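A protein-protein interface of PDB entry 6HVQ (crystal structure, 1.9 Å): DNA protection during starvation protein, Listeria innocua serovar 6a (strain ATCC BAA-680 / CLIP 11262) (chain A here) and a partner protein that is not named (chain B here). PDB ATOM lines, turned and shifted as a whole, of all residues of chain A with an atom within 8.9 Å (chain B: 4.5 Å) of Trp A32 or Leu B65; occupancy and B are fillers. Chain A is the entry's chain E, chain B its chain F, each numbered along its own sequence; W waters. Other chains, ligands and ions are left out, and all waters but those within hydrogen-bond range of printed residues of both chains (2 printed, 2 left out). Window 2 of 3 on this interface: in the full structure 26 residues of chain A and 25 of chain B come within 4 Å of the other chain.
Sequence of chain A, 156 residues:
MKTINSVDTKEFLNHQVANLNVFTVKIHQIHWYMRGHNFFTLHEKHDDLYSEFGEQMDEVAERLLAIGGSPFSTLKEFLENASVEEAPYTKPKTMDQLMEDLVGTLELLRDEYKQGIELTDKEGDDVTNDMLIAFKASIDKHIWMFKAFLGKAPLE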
ATOM      1  N   THR A  24     -19.189  -5.272 -17.767  1.00  0.00           N
ATOM      2  CA  THR A  24     -18.609  -5.778 -16.526  1.00  0.00           C
ATOM      3  C   THR A  24     -19.634  -6.598 -15.748  1.00  0.00           C
ATOM      4  O   THR A  24     -19.295  -7.628 -15.139  1.00  0.00           O
ATOM      5  CB  THR A  24     -18.066  -4.626 -15.674  1.00  0.00           C
ATOM      6  OG1 THR A  24     -19.065  -3.615 -15.519  1.00  0.00           O
ATOM      7  CG2 THR A  24     -16.825  -4.011 -16.318  1.00  0.00           C
ATOM      8  N   VAL A  25     -20.903  -6.178 -15.767  1.00  0.00           N
ATOM      9  CA  VAL A  25     -21.911  -7.020 -15.117  1.00  0.00           C
ATOM     10  C   VAL A  25     -22.031  -8.374 -15.828  1.00  0.00           C
ATOM     11  O   VAL A  25     -22.174  -9.421 -15.179  1.00  0.00           O
ATOM     12  CB  VAL A  25     -23.253  -6.275 -15.022  1.00  0.00           C
ATOM     13  CG1 VAL A  25     -24.360  -7.195 -14.504  1.00  0.00           C
ATOM     14  CG2 VAL A  25     -23.091  -5.075 -14.096  1.00  0.00           C
ATOM     15  N   LYS A  26     -21.949  -8.387 -17.168  1.00  0.00           N
ATOM     16  CA  LYS A  26     -21.976  -9.666 -17.887  1.00  0.00           C
ATOM     17  C   LYS A  26     -20.790 -10.548 -17.496  1.00  0.00           C
ATOM     18  O   LYS A  26     -20.930 -11.773 -17.339  1.00  0.00           O
ATOM     19  CB  LYS A  26     -21.991  -9.423 -19.400  1.00  0.00           C
ATOM     20  CG  LYS A  26     -22.049 -10.694 -20.249  1.00  0.00           C
ATOM     21  CD  LYS A  26     -21.837 -10.426 -21.744  1.00  0.00           C
ATOM     22  CE  LYS A  26     -23.000  -9.676 -22.383  1.00  0.00           C
ATOM     23  NZ  LYS A  26     -24.221 -10.520 -22.491  1.00  0.00           N
ATOM     24  N   ILE A  27     -19.609  -9.947 -17.342  1.00  0.00           N
ATOM     25  CA  ILE A  27     -18.436 -10.715 -16.940  1.00  0.00           C
ATOM     26  C   ILE A  27     -18.680 -11.369 -15.586  1.00  0.00           C
ATOM     27  O   ILE A  27     -18.298 -12.524 -15.361  1.00  0.00           O
ATOM     28  CB  ILE A  27     -17.182  -9.817 -16.930  1.00  0.00           C
ATOM     29  CG1 ILE A  27     -16.829  -9.379 -18.346  1.00  0.00           C
ATOM     30  CG2 ILE A  27     -15.991 -10.550 -16.341  1.00  0.00           C
ATOM     31  CD1 ILE A  27     -15.797  -8.274 -18.406  1.00  0.00           C
ATOM     32  N   HIS A  28     -19.322 -10.646 -14.658  1.00  0.00           N
ATOM     33  CA  HIS A  28     -19.651 -11.269 -13.376  1.00  0.00           C
ATOM     34  C   HIS A  28     -20.661 -12.397 -13.536  1.00  0.00           C
ATOM     35  O   HIS A  28     -20.535 -13.436 -12.883  1.00  0.00           O
ATOM     36  CB  HIS A  28     -20.189 -10.230 -12.391  1.00  0.00           C
ATOM     37  CG  HIS A  28     -19.155  -9.686 -11.460  1.00  0.00           C
ATOM     38  ND1 HIS A  28     -17.954 -10.319 -11.223  1.00  0.00           N
ATOM     39  CD2 HIS A  28     -19.144  -8.566 -10.700  1.00  0.00           C
ATOM     40  CE1 HIS A  28     -17.248  -9.612 -10.360  1.00  0.00           C
ATOM     41  NE2 HIS A  28     -17.948  -8.543 -10.026  1.00  0.00           N
ATOM     42  N   GLN A  29     -21.680 -12.211 -14.381  1.00  0.00           N
ATOM     43  CA  GLN A  29     -22.631 -13.292 -14.641  1.00  0.00           C
ATOM     44  C   GLN A  29     -21.912 -14.573 -15.050  1.00  0.00           C
ATOM     45  O   GLN A  29     -22.194 -15.661 -14.528  1.00  0.00           O
ATOM     46  CB  GLN A  29     -23.624 -12.863 -15.726  1.00  0.00           C
ATOM     47  CG  GLN A  29     -24.634 -13.932 -16.134  1.00  0.00           C
ATOM     48  CD  GLN A  29     -25.566 -13.451 -17.229  1.00  0.00           C
ATOM     49  OE1 GLN A  29     -25.260 -13.574 -18.412  1.00  0.00           O
ATOM     50  NE2 GLN A  29     -26.722 -12.922 -16.840  1.00  0.00           N
ATOM     51  N   ILE A  30     -20.980 -14.458 -15.997  1.00  0.00           N
ATOM     52  CA  ILE A  30     -20.238 -15.628 -16.461  1.00  0.00           C
ATOM     53  C   ILE A  30     -19.379 -16.199 -15.336  1.00  0.00           C
ATOM     54  O   ILE A  30     -19.307 -17.418 -15.136  1.00  0.00           O
ATOM     55  CB  ILE A  30     -19.400 -15.256 -17.698  1.00  0.00           C
ATOM     56  CG1 ILE A  30     -20.333 -14.861 -18.848  1.00  0.00           C
ATOM     57  CG2 ILE A  30     -18.512 -16.417 -18.107  1.00  0.00           C
ATOM     58  CD1 ILE A  30     -19.640 -14.198 -20.013  1.00  0.00           C
ATOM     59  N   HIS A  31     -18.687 -15.320 -14.609  1.00  0.00           N
ATOM     60  CA  HIS A  31     -17.872 -15.725 -13.464  1.00  0.00           C
ATOM     61  C   HIS A  31     -18.675 -16.581 -12.479  1.00  0.00           C
ATOM     62  O   HIS A  31     -18.209 -17.634 -12.021  1.00  0.00           O
ATOM     63  CB  HIS A  31     -17.332 -14.449 -12.805  1.00  0.00           C
ATOM     64  CG  HIS A  31     -16.499 -14.662 -11.578  1.00  0.00           C
ATOM     65  ND1 HIS A  31     -15.177 -15.059 -11.622  1.00  0.00           N
ATOM     66  CD2 HIS A  31     -16.786 -14.461 -10.269  1.00  0.00           C
ATOM     67  CE1 HIS A  31     -14.697 -15.124 -10.392  1.00  0.00           C
ATOM     68  NE2 HIS A  31     -15.655 -14.772  -9.551  1.00  0.00           N
ATOM     69  N   TRP A  32     -19.901 -16.154 -12.168  1.00  0.00           N
ATOM     70  CA  TRP A  32     -20.721 -16.808 -11.150  1.00  0.00           C
ATOM     71  C   TRP A  32     -21.360 -18.100 -11.651  1.00  0.00           C
ATOM     72  O   TRP A  32     -21.423 -19.090 -10.909  1.00  0.00           O
ATOM     73  CB  TRP A  32     -21.822 -15.851 -10.677  1.00  0.00           C
ATOM     74  CG  TRP A  32     -21.330 -14.679  -9.894  1.00  0.00           C
ATOM     75  CD1 TRP A  32     -20.184 -14.602  -9.157  1.00  0.00           C
ATOM     76  CD2 TRP A  32     -21.970 -13.403  -9.779  1.00  0.00           C
ATOM     77  NE1 TRP A  32     -20.072 -13.357  -8.582  1.00  0.00           N
ATOM     78  CE2 TRP A  32     -21.157 -12.602  -8.945  1.00  0.00           C
ATOM     79  CE3 TRP A  32     -23.151 -12.862 -10.294  1.00  0.00           C
ATOM     80  CZ2 TRP A  32     -21.481 -11.284  -8.629  1.00  0.00           C
ATOM     81  CZ3 TRP A  32     -23.483 -11.552  -9.968  1.00  0.00           C
ATOM     82  CH2 TRP A  32     -22.644 -10.774  -9.150  1.00  0.00           C
ATOM     83  N   TYR A  33     -21.869 -18.111 -12.884  1.00  0.00           N
ATOM     84  CA  TYR A  33     -22.742 -19.201 -13.326  1.00  0.00           C
ATOM     85  C   TYR A  33     -22.042 -20.302 -14.114  1.00  0.00           C
ATOM     86  O   TYR A  33     -22.663 -21.337 -14.377  1.00  0.00           O
ATOM     87  CB  TYR A  33     -23.893 -18.637 -14.173  1.00  0.00           C
ATOM     88  CG  TYR A  33     -25.019 -18.065 -13.344  1.00  0.00           C
ATOM     89  CD1 TYR A  33     -25.938 -18.900 -12.724  1.00  0.00           C
ATOM     90  CD2 TYR A  33     -25.166 -16.695 -13.177  1.00  0.00           C
ATOM     91  CE1 TYR A  33     -26.976 -18.388 -11.964  1.00  0.00           C
ATOM     92  CE2 TYR A  33     -26.206 -16.172 -12.414  1.00  0.00           C
ATOM     93  CZ  TYR A  33     -27.103 -17.020 -11.811  1.00  0.00           C
ATOM     94  OH  TYR A  33     -28.139 -16.508 -11.055  1.00  0.00           O
ATOM     95  N   MET A  34     -20.780 -20.124 -14.486  1.00  0.00           N
ATOM     96  CA  MET A  34     -20.095 -21.102 -15.320  1.00  0.00           C
ATOM     97  C   MET A  34     -19.976 -22.460 -14.628  1.00  0.00           C
ATOM     98  O   MET A  34     -19.835 -22.558 -13.405  1.00  0.00           O
ATOM     99  CB  MET A  34     -18.701 -20.594 -15.682  1.00  0.00           C
ATOM    100  CG  MET A  34     -17.834 -20.245 -14.483  1.00  0.00           C
ATOM    101  SD  MET A  34     -16.105 -20.017 -14.938  1.00  0.00           S
ATOM    102  CE  MET A  34     -16.284 -18.793 -16.227  1.00  0.00           C
ATOM    103  N   ARG A  35     -20.035 -23.519 -15.438  1.00  0.00           N
ATOM    104  CA  ARG A  35     -19.790 -24.884 -14.983  1.00  0.00           C
ATOM    105  C   ARG A  35     -19.013 -25.642 -16.054  1.00  0.00           C
ATOM    106  O   ARG A  35     -19.029 -25.277 -17.229  1.00  0.00           O
ATOM    107  CB  ARG A  35     -21.094 -25.636 -14.683  1.00  0.00           C
ATOM    108  CG  ARG A  35     -21.917 -25.049 -13.556  1.00  0.00           C
ATOM    109  CD  ARG A  35     -23.168 -25.877 -13.340  1.00  0.00           C
ATOM    110  NE  ARG A  35     -24.024 -25.316 -12.302  1.00  0.00           N
ATOM    111  CZ  ARG A  35     -25.239 -25.766 -12.019  1.00  0.00           C
ATOM    112  NH1 ARG A  35     -25.742 -26.792 -12.696  1.00  0.00           N
ATOM    113  NH2 ARG A  35     -25.949 -25.194 -11.055  1.00  0.00           N
ATOM    114  N   PHE A  39     -13.654 -24.889 -15.314  1.00  0.00           N
ATOM    115  CA  PHE A  39     -14.160 -23.905 -14.362  1.00  0.00           C
ATOM    116  C   PHE A  39     -13.051 -23.047 -13.765  1.00  0.00           C
ATOM    117  O   PHE A  39     -13.130 -21.821 -13.800  1.00  0.00           O
ATOM    118  CB  PHE A  39     -14.941 -24.586 -13.237  1.00  0.00           C
ATOM    119  CG  PHE A  39     -15.382 -23.626 -12.157  1.00  0.00           C
ATOM    120  CD1 PHE A  39     -16.584 -22.954 -12.264  1.00  0.00           C
ATOM    121  CD2 PHE A  39     -14.576 -23.372 -11.060  1.00  0.00           C
ATOM    122  CE1 PHE A  39     -16.990 -22.066 -11.282  1.00  0.00           C
ATOM    123  CE2 PHE A  39     -14.970 -22.481 -10.076  1.00  0.00           C
ATOM    124  CZ  PHE A  39     -16.173 -21.829 -10.184  1.00  0.00           C
ATOM    125  N   LEU A  42     -11.079 -20.417 -16.156  1.00  0.00           N
ATOM    126  CA  LEU A  42     -11.892 -19.337 -16.708  1.00  0.00           C
ATOM    127  C   LEU A  42     -12.536 -18.505 -15.612  1.00  0.00           C
ATOM    128  O   LEU A  42     -12.749 -17.300 -15.794  1.00  0.00           O
ATOM    129  CB  LEU A  42     -12.953 -19.916 -17.639  1.00  0.00           C
ATOM    130  CG  LEU A  42     -12.387 -20.402 -18.968  1.00  0.00           C
ATOM    131  CD1 LEU A  42     -13.422 -21.172 -19.746  1.00  0.00           C
ATOM    132  CD2 LEU A  42     -11.921 -19.204 -19.782  1.00  0.00           C
ATOM    133  N   HIS A  43     -12.834 -19.127 -14.472  1.00  0.00           N
ATOM    134  CA  HIS A  43     -13.340 -18.394 -13.319  1.00  0.00           C
ATOM    135  C   HIS A  43     -12.380 -17.281 -12.935  1.00  0.00           C
ATOM    136  O   HIS A  43     -12.782 -16.120 -12.809  1.00  0.00           O
ATOM    137  CB  HIS A  43     -13.565 -19.366 -12.155  1.00  0.00           C
ATOM    138  CG  HIS A  43     -14.322 -18.783 -11.001  1.00  0.00           C
ATOM    139  ND1 HIS A  43     -15.643 -18.397 -11.097  1.00  0.00           N
ATOM    140  CD2 HIS A  43     -13.964 -18.579  -9.710  1.00  0.00           C
ATOM    141  CE1 HIS A  43     -16.054 -17.947  -9.924  1.00  0.00           C
ATOM    142  NE2 HIS A  43     -15.054 -18.050  -9.064  1.00  0.00           N
ATOM    143  N   HIS A  46     -12.069 -14.406 -15.623  1.00  0.00           N
ATOM    144  CA  HIS A  46     -13.084 -13.361 -15.656  1.00  0.00           C
ATOM    145  C   HIS A  46     -12.839 -12.291 -14.602  1.00  0.00           C
ATOM    146  O   HIS A  46     -13.247 -11.143 -14.795  1.00  0.00           O
ATOM    147  CB  HIS A  46     -14.466 -13.976 -15.510  1.00  0.00           C
ATOM    148  CG  HIS A  46     -14.924 -14.655 -16.754  1.00  0.00           C
ATOM    149  ND1 HIS A  46     -15.111 -13.985 -17.942  1.00  0.00           N
ATOM    150  CD2 HIS A  46     -15.170 -15.955 -17.013  1.00  0.00           C
ATOM    151  CE1 HIS A  46     -15.483 -14.836 -18.871  1.00  0.00           C
ATOM    152  NE2 HIS A  46     -15.524 -16.042 -18.338  1.00  0.00           N
ATOM    153  N   ASP A  47     -12.176 -12.636 -13.493  1.00  0.00           N
ATOM    154  CA  ASP A  47     -11.726 -11.590 -12.579  1.00  0.00           C
ATOM    155  C   ASP A  47     -10.747 -10.667 -13.291  1.00  0.00           C
ATOM    156  O   ASP A  47     -10.811  -9.434 -13.144  1.00  0.00           O
ATOM    157  CB  ASP A  47     -11.066 -12.194 -11.337  1.00  0.00           C
ATOM    158  CG  ASP A  47     -12.074 -12.658 -10.306  1.00  0.00           C
ATOM    159  OD1 ASP A  47     -13.232 -12.194 -10.365  1.00  0.00           O
ATOM    160  OD2 ASP A  47     -11.711 -13.477  -9.431  1.00  0.00           O
ATOM    161  N   TYR A  50     -12.826  -8.438 -15.598  1.00  0.00           N
ATOM    162  CA  TYR A  50     -13.610  -7.487 -14.819  1.00  0.00           C
ATOM    163  C   TYR A  50     -12.752  -6.298 -14.404  1.00  0.00           C
ATOM    164  O   TYR A  50     -13.140  -5.136 -14.597  1.00  0.00           O
ATOM    165  CB  TYR A  50     -14.200  -8.190 -13.595  1.00  0.00           C
ATOM    166  CG  TYR A  50     -15.192  -7.358 -12.811  1.00  0.00           C
ATOM    167  CD1 TYR A  50     -16.527  -7.300 -13.185  1.00  0.00           C
ATOM    168  CD2 TYR A  50     -14.794  -6.637 -11.690  1.00  0.00           C
ATOM    169  CE1 TYR A  50     -17.439  -6.547 -12.469  1.00  0.00           C
ATOM    170  CE2 TYR A  50     -15.701  -5.878 -10.968  1.00  0.00           C
ATOM    171  CZ  TYR A  50     -17.022  -5.838 -11.363  1.00  0.00           C
ATOM    172  OH  TYR A  50     -17.933  -5.090 -10.651  1.00  0.00           O
ATOM    173  N   TYR A  89     -29.791 -15.020 -16.515  1.00  0.00           N
ATOM    174  CA  TYR A  89     -29.386 -16.421 -16.597  1.00  0.00           C
ATOM    175  C   TYR A  89     -30.544 -17.277 -16.107  1.00  0.00           C
ATOM    176  O   TYR A  89     -30.798 -17.369 -14.904  1.00  0.00           O
ATOM    177  CB  TYR A  89     -28.122 -16.675 -15.785  1.00  0.00           C
ATOM    178  CG  TYR A  89     -27.500 -18.014 -16.098  1.00  0.00           C
ATOM    179  CD1 TYR A  89     -26.470 -18.123 -17.023  1.00  0.00           C
ATOM    180  CD2 TYR A  89     -27.958 -19.174 -15.488  1.00  0.00           C
ATOM    181  CE1 TYR A  89     -25.906 -19.348 -17.321  1.00  0.00           C
ATOM    182  CE2 TYR A  89     -27.403 -20.399 -15.776  1.00  0.00           C
ATOM    183  CZ  TYR A  89     -26.378 -20.484 -16.695  1.00  0.00           C
ATOM    184  OH  TYR A  89     -25.823 -21.707 -16.983  1.00  0.00           O
ATOM    185  N   LEU A  98     -21.147 -19.513 -23.070  1.00  0.00           N
ATOM    186  CA  LEU A  98     -20.786 -18.325 -22.310  1.00  0.00           C
ATOM    187  C   LEU A  98     -19.614 -17.598 -22.961  1.00  0.00           C
ATOM    188  O   LEU A  98     -19.628 -16.366 -23.091  1.00  0.00           O
ATOM    189  CB  LEU A  98     -20.465 -18.713 -20.866  1.00  0.00           C
ATOM    190  CG  LEU A  98     -21.622 -19.301 -20.049  1.00  0.00           C
ATOM    191  CD1 LEU A  98     -21.143 -19.732 -18.668  1.00  0.00           C
ATOM    192  CD2 LEU A  98     -22.777 -18.321 -19.924  1.00  0.00           C
ATOM    193  N   MET B  57     -20.214  -7.308  -2.675  1.00  0.00           N
ATOM    194  CA  MET B  57     -21.218  -7.780  -3.622  1.00  0.00           C
ATOM    195  C   MET B  57     -20.865  -9.170  -4.138  1.00  0.00           C
ATOM    196  O   MET B  57     -21.711 -10.078  -4.161  1.00  0.00           O
ATOM    197  CB  MET B  57     -21.334  -6.782  -4.772  1.00  0.00           C
ATOM    198  CG  MET B  57     -22.492  -7.024  -5.700  1.00  0.00           C
ATOM    199  SD  MET B  57     -22.027  -8.127  -7.042  1.00  0.00           S
ATOM    200  CE  MET B  57     -20.990  -7.044  -8.020  1.00  0.00           C
ATOM    201  N   ASP B  58     -19.609  -9.355  -4.548  1.00  0.00           N
ATOM    202  CA  ASP B  58     -19.166 -10.660  -5.027  1.00  0.00           C
ATOM    203  C   ASP B  58     -19.319 -11.731  -3.948  1.00  0.00           C
ATOM    204  O   ASP B  58     -19.817 -12.831  -4.217  1.00  0.00           O
ATOM    205  CB  ASP B  58     -17.716 -10.559  -5.503  1.00  0.00           C
ATOM    206  CG  ASP B  58     -17.133 -11.896  -5.911  1.00  0.00           C
ATOM    207  OD1 ASP B  58     -17.710 -12.580  -6.788  1.00  0.00           O
ATOM    208  OD2 ASP B  58     -16.071 -12.257  -5.363  1.00  0.00           O
ATOM    209  N   ALA B  61     -23.044 -12.653  -3.585  1.00  0.00           N
ATOM    210  CA  ALA B  61     -23.520 -13.473  -4.692  1.00  0.00           C
ATOM    211  C   ALA B  61     -23.001 -14.899  -4.581  1.00  0.00           C
ATOM    212  O   ALA B  61     -23.727 -15.861  -4.866  1.00  0.00           O
ATOM    213  CB  ALA B  61     -23.093 -12.853  -6.023  1.00  0.00           C
ATOM    214  N   GLU B  62     -21.742 -15.062  -4.166  1.00  0.00           N
ATOM    215  CA  GLU B  62     -21.161 -16.397  -4.151  1.00  0.00           C
ATOM    216  C   GLU B  62     -21.595 -17.192  -2.926  1.00  0.00           C
ATOM    217  O   GLU B  62     -21.698 -18.427  -2.997  1.00  0.00           O
ATOM    218  CB  GLU B  62     -19.638 -16.284  -4.278  1.00  0.00           C
ATOM    219  CG  GLU B  62     -19.246 -16.058  -5.738  1.00  0.00           C
ATOM    220  CD  GLU B  62     -17.812 -15.611  -5.960  1.00  0.00           C
ATOM    221  OE1 GLU B  62     -17.090 -15.308  -4.985  1.00  0.00           O
ATOM    222  OE2 GLU B  62     -17.404 -15.573  -7.140  1.00  0.00           O
ATOM    223  N   ARG B  63     -21.911 -16.515  -1.820  1.00  0.00           N
ATOM    224  CA  ARG B  63     -22.572 -17.199  -0.713  1.00  0.00           C
ATOM    225  C   ARG B  63     -23.970 -17.657  -1.116  1.00  0.00           C
ATOM    226  O   ARG B  63     -24.387 -18.767  -0.767  1.00  0.00           O
ATOM    227  CB  ARG B  63     -22.645 -16.295   0.515  1.00  0.00           C
ATOM    228  CG  ARG B  63     -23.341 -16.941   1.724  1.00  0.00           C
ATOM    229  CD  ARG B  63     -22.613 -18.190   2.227  1.00  0.00           C
ATOM    230  NE  ARG B  63     -23.427 -18.925   3.190  1.00  0.00           N
ATOM    231  CZ  ARG B  63     -23.204 -20.178   3.569  1.00  0.00           C
ATOM    232  NH1 ARG B  63     -22.181 -20.855   3.079  1.00  0.00           N
ATOM    233  NH2 ARG B  63     -24.017 -20.759   4.435  1.00  0.00           N
ATOM    234  N   LEU B  64     -24.713 -16.815  -1.842  1.00  0.00           N
ATOM    235  CA  LEU B  64     -26.015 -17.241  -2.354  1.00  0.00           C
ATOM    236  C   LEU B  64     -25.874 -18.483  -3.223  1.00  0.00           C
ATOM    237  O   LEU B  64     -26.666 -19.428  -3.100  1.00  0.00           O
ATOM    238  CB  LEU B  64     -26.675 -16.109  -3.142  1.00  0.00           C
ATOM    239  CG  LEU B  64     -28.036 -16.433  -3.783  1.00  0.00           C
ATOM    240  CD1 LEU B  64     -29.044 -16.924  -2.754  1.00  0.00           C
ATOM    241  CD2 LEU B  64     -28.573 -15.219  -4.535  1.00  0.00           C
ATOM    242  N   LEU B  65     -24.868 -18.504  -4.103  1.00  0.00           N
ATOM    243  CA  LEU B  65     -24.611 -19.706  -4.891  1.00  0.00           C
ATOM    244  C   LEU B  65     -24.349 -20.908  -3.996  1.00  0.00           C
ATOM    245  O   LEU B  65     -24.872 -22.000  -4.242  1.00  0.00           O
ATOM    246  CB  LEU B  65     -23.416 -19.491  -5.820  1.00  0.00           C
ATOM    247  CG  LEU B  65     -23.583 -18.621  -7.058  1.00  0.00           C
ATOM    248  CD1 LEU B  65     -22.215 -18.249  -7.600  1.00  0.00           C
ATOM    249  CD2 LEU B  65     -24.369 -19.388  -8.112  1.00  0.00           C
ATOM    250  N   ALA B  66     -23.531 -20.730  -2.958  1.00  0.00           N
ATOM    251  CA  ALA B  66     -23.111 -21.864  -2.149  1.00  0.00           C
ATOM    252  C   ALA B  66     -24.251 -22.449  -1.323  1.00  0.00           C
ATOM    253  O   ALA B  66     -24.150 -23.607  -0.898  1.00  0.00           O
ATOM    254  CB  ALA B  66     -21.951 -21.453  -1.235  1.00  0.00           C
ATOM    255  N   ILE B  67     -25.320 -21.686  -1.078  1.00  0.00           N
ATOM    256  CA  ILE B  67     -26.482 -22.212  -0.367  1.00  0.00           C
ATOM    257  C   ILE B  67     -27.582 -22.647  -1.329  1.00  0.00           C
ATOM    258  O   ILE B  67     -28.707 -22.928  -0.897  1.00  0.00           O
ATOM    259  CB  ILE B  67     -27.034 -21.212   0.667  1.00  0.00           C
ATOM    260  CG1 ILE B  67     -27.549 -19.934  -0.005  1.00  0.00           C
ATOM    261  CG2 ILE B  67     -25.964 -20.876   1.704  1.00  0.00           C
ATOM    262  CD1 ILE B  67     -28.244 -18.971   0.962  1.00  0.00           C
ATOM    263  N   GLY B  68     -27.280 -22.731  -2.621  1.00  0.00           N
ATOM    264  CA  GLY B  68     -28.207 -23.259  -3.598  1.00  0.00           C
ATOM    265  C   GLY B  68     -29.018 -22.231  -4.353  1.00  0.00           C
ATOM    266  O   GLY B  68     -29.996 -22.609  -5.008  1.00  0.00           O
ATOM    267  N   GLY B  69     -28.648 -20.952  -4.287  1.00  0.00           N
ATOM    268  CA  GLY B  69     -29.394 -19.894  -4.927  1.00  0.00           C
ATOM    269  C   GLY B  69     -28.812 -19.451  -6.265  1.00  0.00           C
ATOM    270  O   GLY B  69     -27.825 -19.981  -6.770  1.00  0.00           O
ATOM    271  N   PRO B  71     -27.942 -15.785  -8.173  1.00  0.00           N
ATOM    272  CA  PRO B  71     -27.873 -14.323  -8.027  1.00  0.00           C
ATOM    273  C   PRO B  71     -28.391 -13.575  -9.247  1.00  0.00           C
ATOM    274  O   PRO B  71     -28.202 -13.999 -10.391  1.00  0.00           O
ATOM    275  CB  PRO B  71     -26.374 -14.061  -7.828  1.00  0.00           C
ATOM    276  CG  PRO B  71     -25.706 -15.204  -8.503  1.00  0.00           C
ATOM    277  CD  PRO B  71     -26.600 -16.387  -8.278  1.00  0.00           C
ATOM    278  N   PHE B  72     -29.057 -12.447  -8.991  1.00  0.00           N
ATOM    279  CA  PHE B  72     -29.292 -11.472 -10.047  1.00  0.00           C
ATOM    280  C   PHE B  72     -27.964 -11.150 -10.718  1.00  0.00           C
ATOM    281  O   PHE B  72     -26.927 -11.061 -10.056  1.00  0.00           O
ATOM    282  CB  PHE B  72     -29.900 -10.185  -9.480  1.00  0.00           C
ATOM    283  CG  PHE B  72     -31.225 -10.371  -8.791  1.00  0.00           C
ATOM    284  CD1 PHE B  72     -32.245 -11.097  -9.375  1.00  0.00           C
ATOM    285  CD2 PHE B  72     -31.454  -9.779  -7.558  1.00  0.00           C
ATOM    286  CE1 PHE B  72     -33.462 -11.243  -8.737  1.00  0.00           C
ATOM    287  CE2 PHE B  72     -32.667  -9.922  -6.920  1.00  0.00           C
ATOM    288  CZ  PHE B  72     -33.672 -10.657  -7.511  1.00  0.00           C
ATOM    289  N   SER B  73     -27.991 -10.951 -12.045  1.00  0.00           N
ATOM    290  CA  SER B  73     -26.742 -10.772 -12.782  1.00  0.00           C
ATOM    291  C   SER B  73     -26.923  -9.935 -14.043  1.00  0.00           C
ATOM    292  O   SER B  73     -26.194 -10.126 -15.025  1.00  0.00           O
ATOM    293  CB  SER B  73     -26.151 -12.137 -13.137  1.00  0.00           C
ATOM    294  OG  SER B  73     -27.044 -12.877 -13.969  1.00  0.00           O
HETATM  295  O   HOH W   1     -25.328  -9.874 -17.774  1.00  0.00           O
HETATM  296  O   HOH W   2     -29.591 -13.517 -13.887  1.00  0.00           O
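Of the 14 printed residues of chain B, 8 touch a printed residue of chain A.
Printed residues of chain B that touch a printed residue of chain A: Met B57, Asp B58, Ala B61, Glu B62, Leu B65, Pro B71, Phe B72 and Ser B73.
Among the printed residues, 14 pairs touch across the chains.
Among the printed residues, no Asp or Glu carboxylate lies within 4 Å of a Lys or Arg side-chain nitrogen of the other chain.
Of chain B, only Met B57, Asp B58, Ala B61, Glu B62, Leu B65, Pro B71 and Phe B72 come within 4 Å of Trp A32.
Of chain A, only Trp A32 (3.5 Å) comes within 4 Å of Leu B65.
No residue of chain A comes within 4 Å of Ala B66.
No residue of chain A comes within 4 Å of Gly B69.
Of the printed residues of chain A, Ala B61 touches Trp A32 (3.4 Å).
Of the printed residues of chain A, Glu B62 touches His A31 (3.1 Å), Trp A32 (3.6 Å) and His A43 (3.9 Å).
The nearest residue of chain A that does not touch Leu B65 is Tyr A33 (4.8 Å).
ND1 of His A43 sits at hydrogen-bond distance from O of His A31, at 2.8 Å.
The side-chain sulfur (SD) of Met A34 is in hydrogen-bond range of the backbone NH (N) of His A43 (3.4 Å).
Water W2 lies within hydrogen-bond range of the side-chain hydroxyl (OG) of Ser B73 (2.6 Å) and the backbone NH (N) of Tyr A89 (3.0 Å).
Water W1 bridges O of Ser B73 (2.9 Å) and NE2 of Gln A29 (3.5 Å).
CG1 of Val A25 touches O of Ser B73, at 3.5 Å.
Met B57 touches His A28 (CE to CD2, 3.6 Å).
Trp A32 touches Met B57 (CH2 to SD, 3.4 Å).
Ala B61 touches Trp A32.
Glu B62 touches Trp A32.
Trp A32 touches Leu B65 (O to CD1, 3.5 Å).
CG of Pro B71 touches CE3 of Trp A32, 3.9 Å away.
Trp A32 touches Phe B72 (CZ3 to O, 3.5 Å).
Tyr A33 touches Ser B73.
His A43 touches Glu B62.
The indole nitrogen of Trp A32 sits at hydrogen-bond distance from the side-chain carboxylate of Asp B58.
The side-chain carboxylate (OE2) of Glu B62 lies close to a ring nitrogen (NE2) of His A31 (3.1 Å).
OH of Tyr A33 lies within hydrogen-bond range of O of Pro B71, at 2.6 Å.
NE2 of Gln A29 is in hydrogen-bond range of OG of Ser B73 (2.9 Å).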
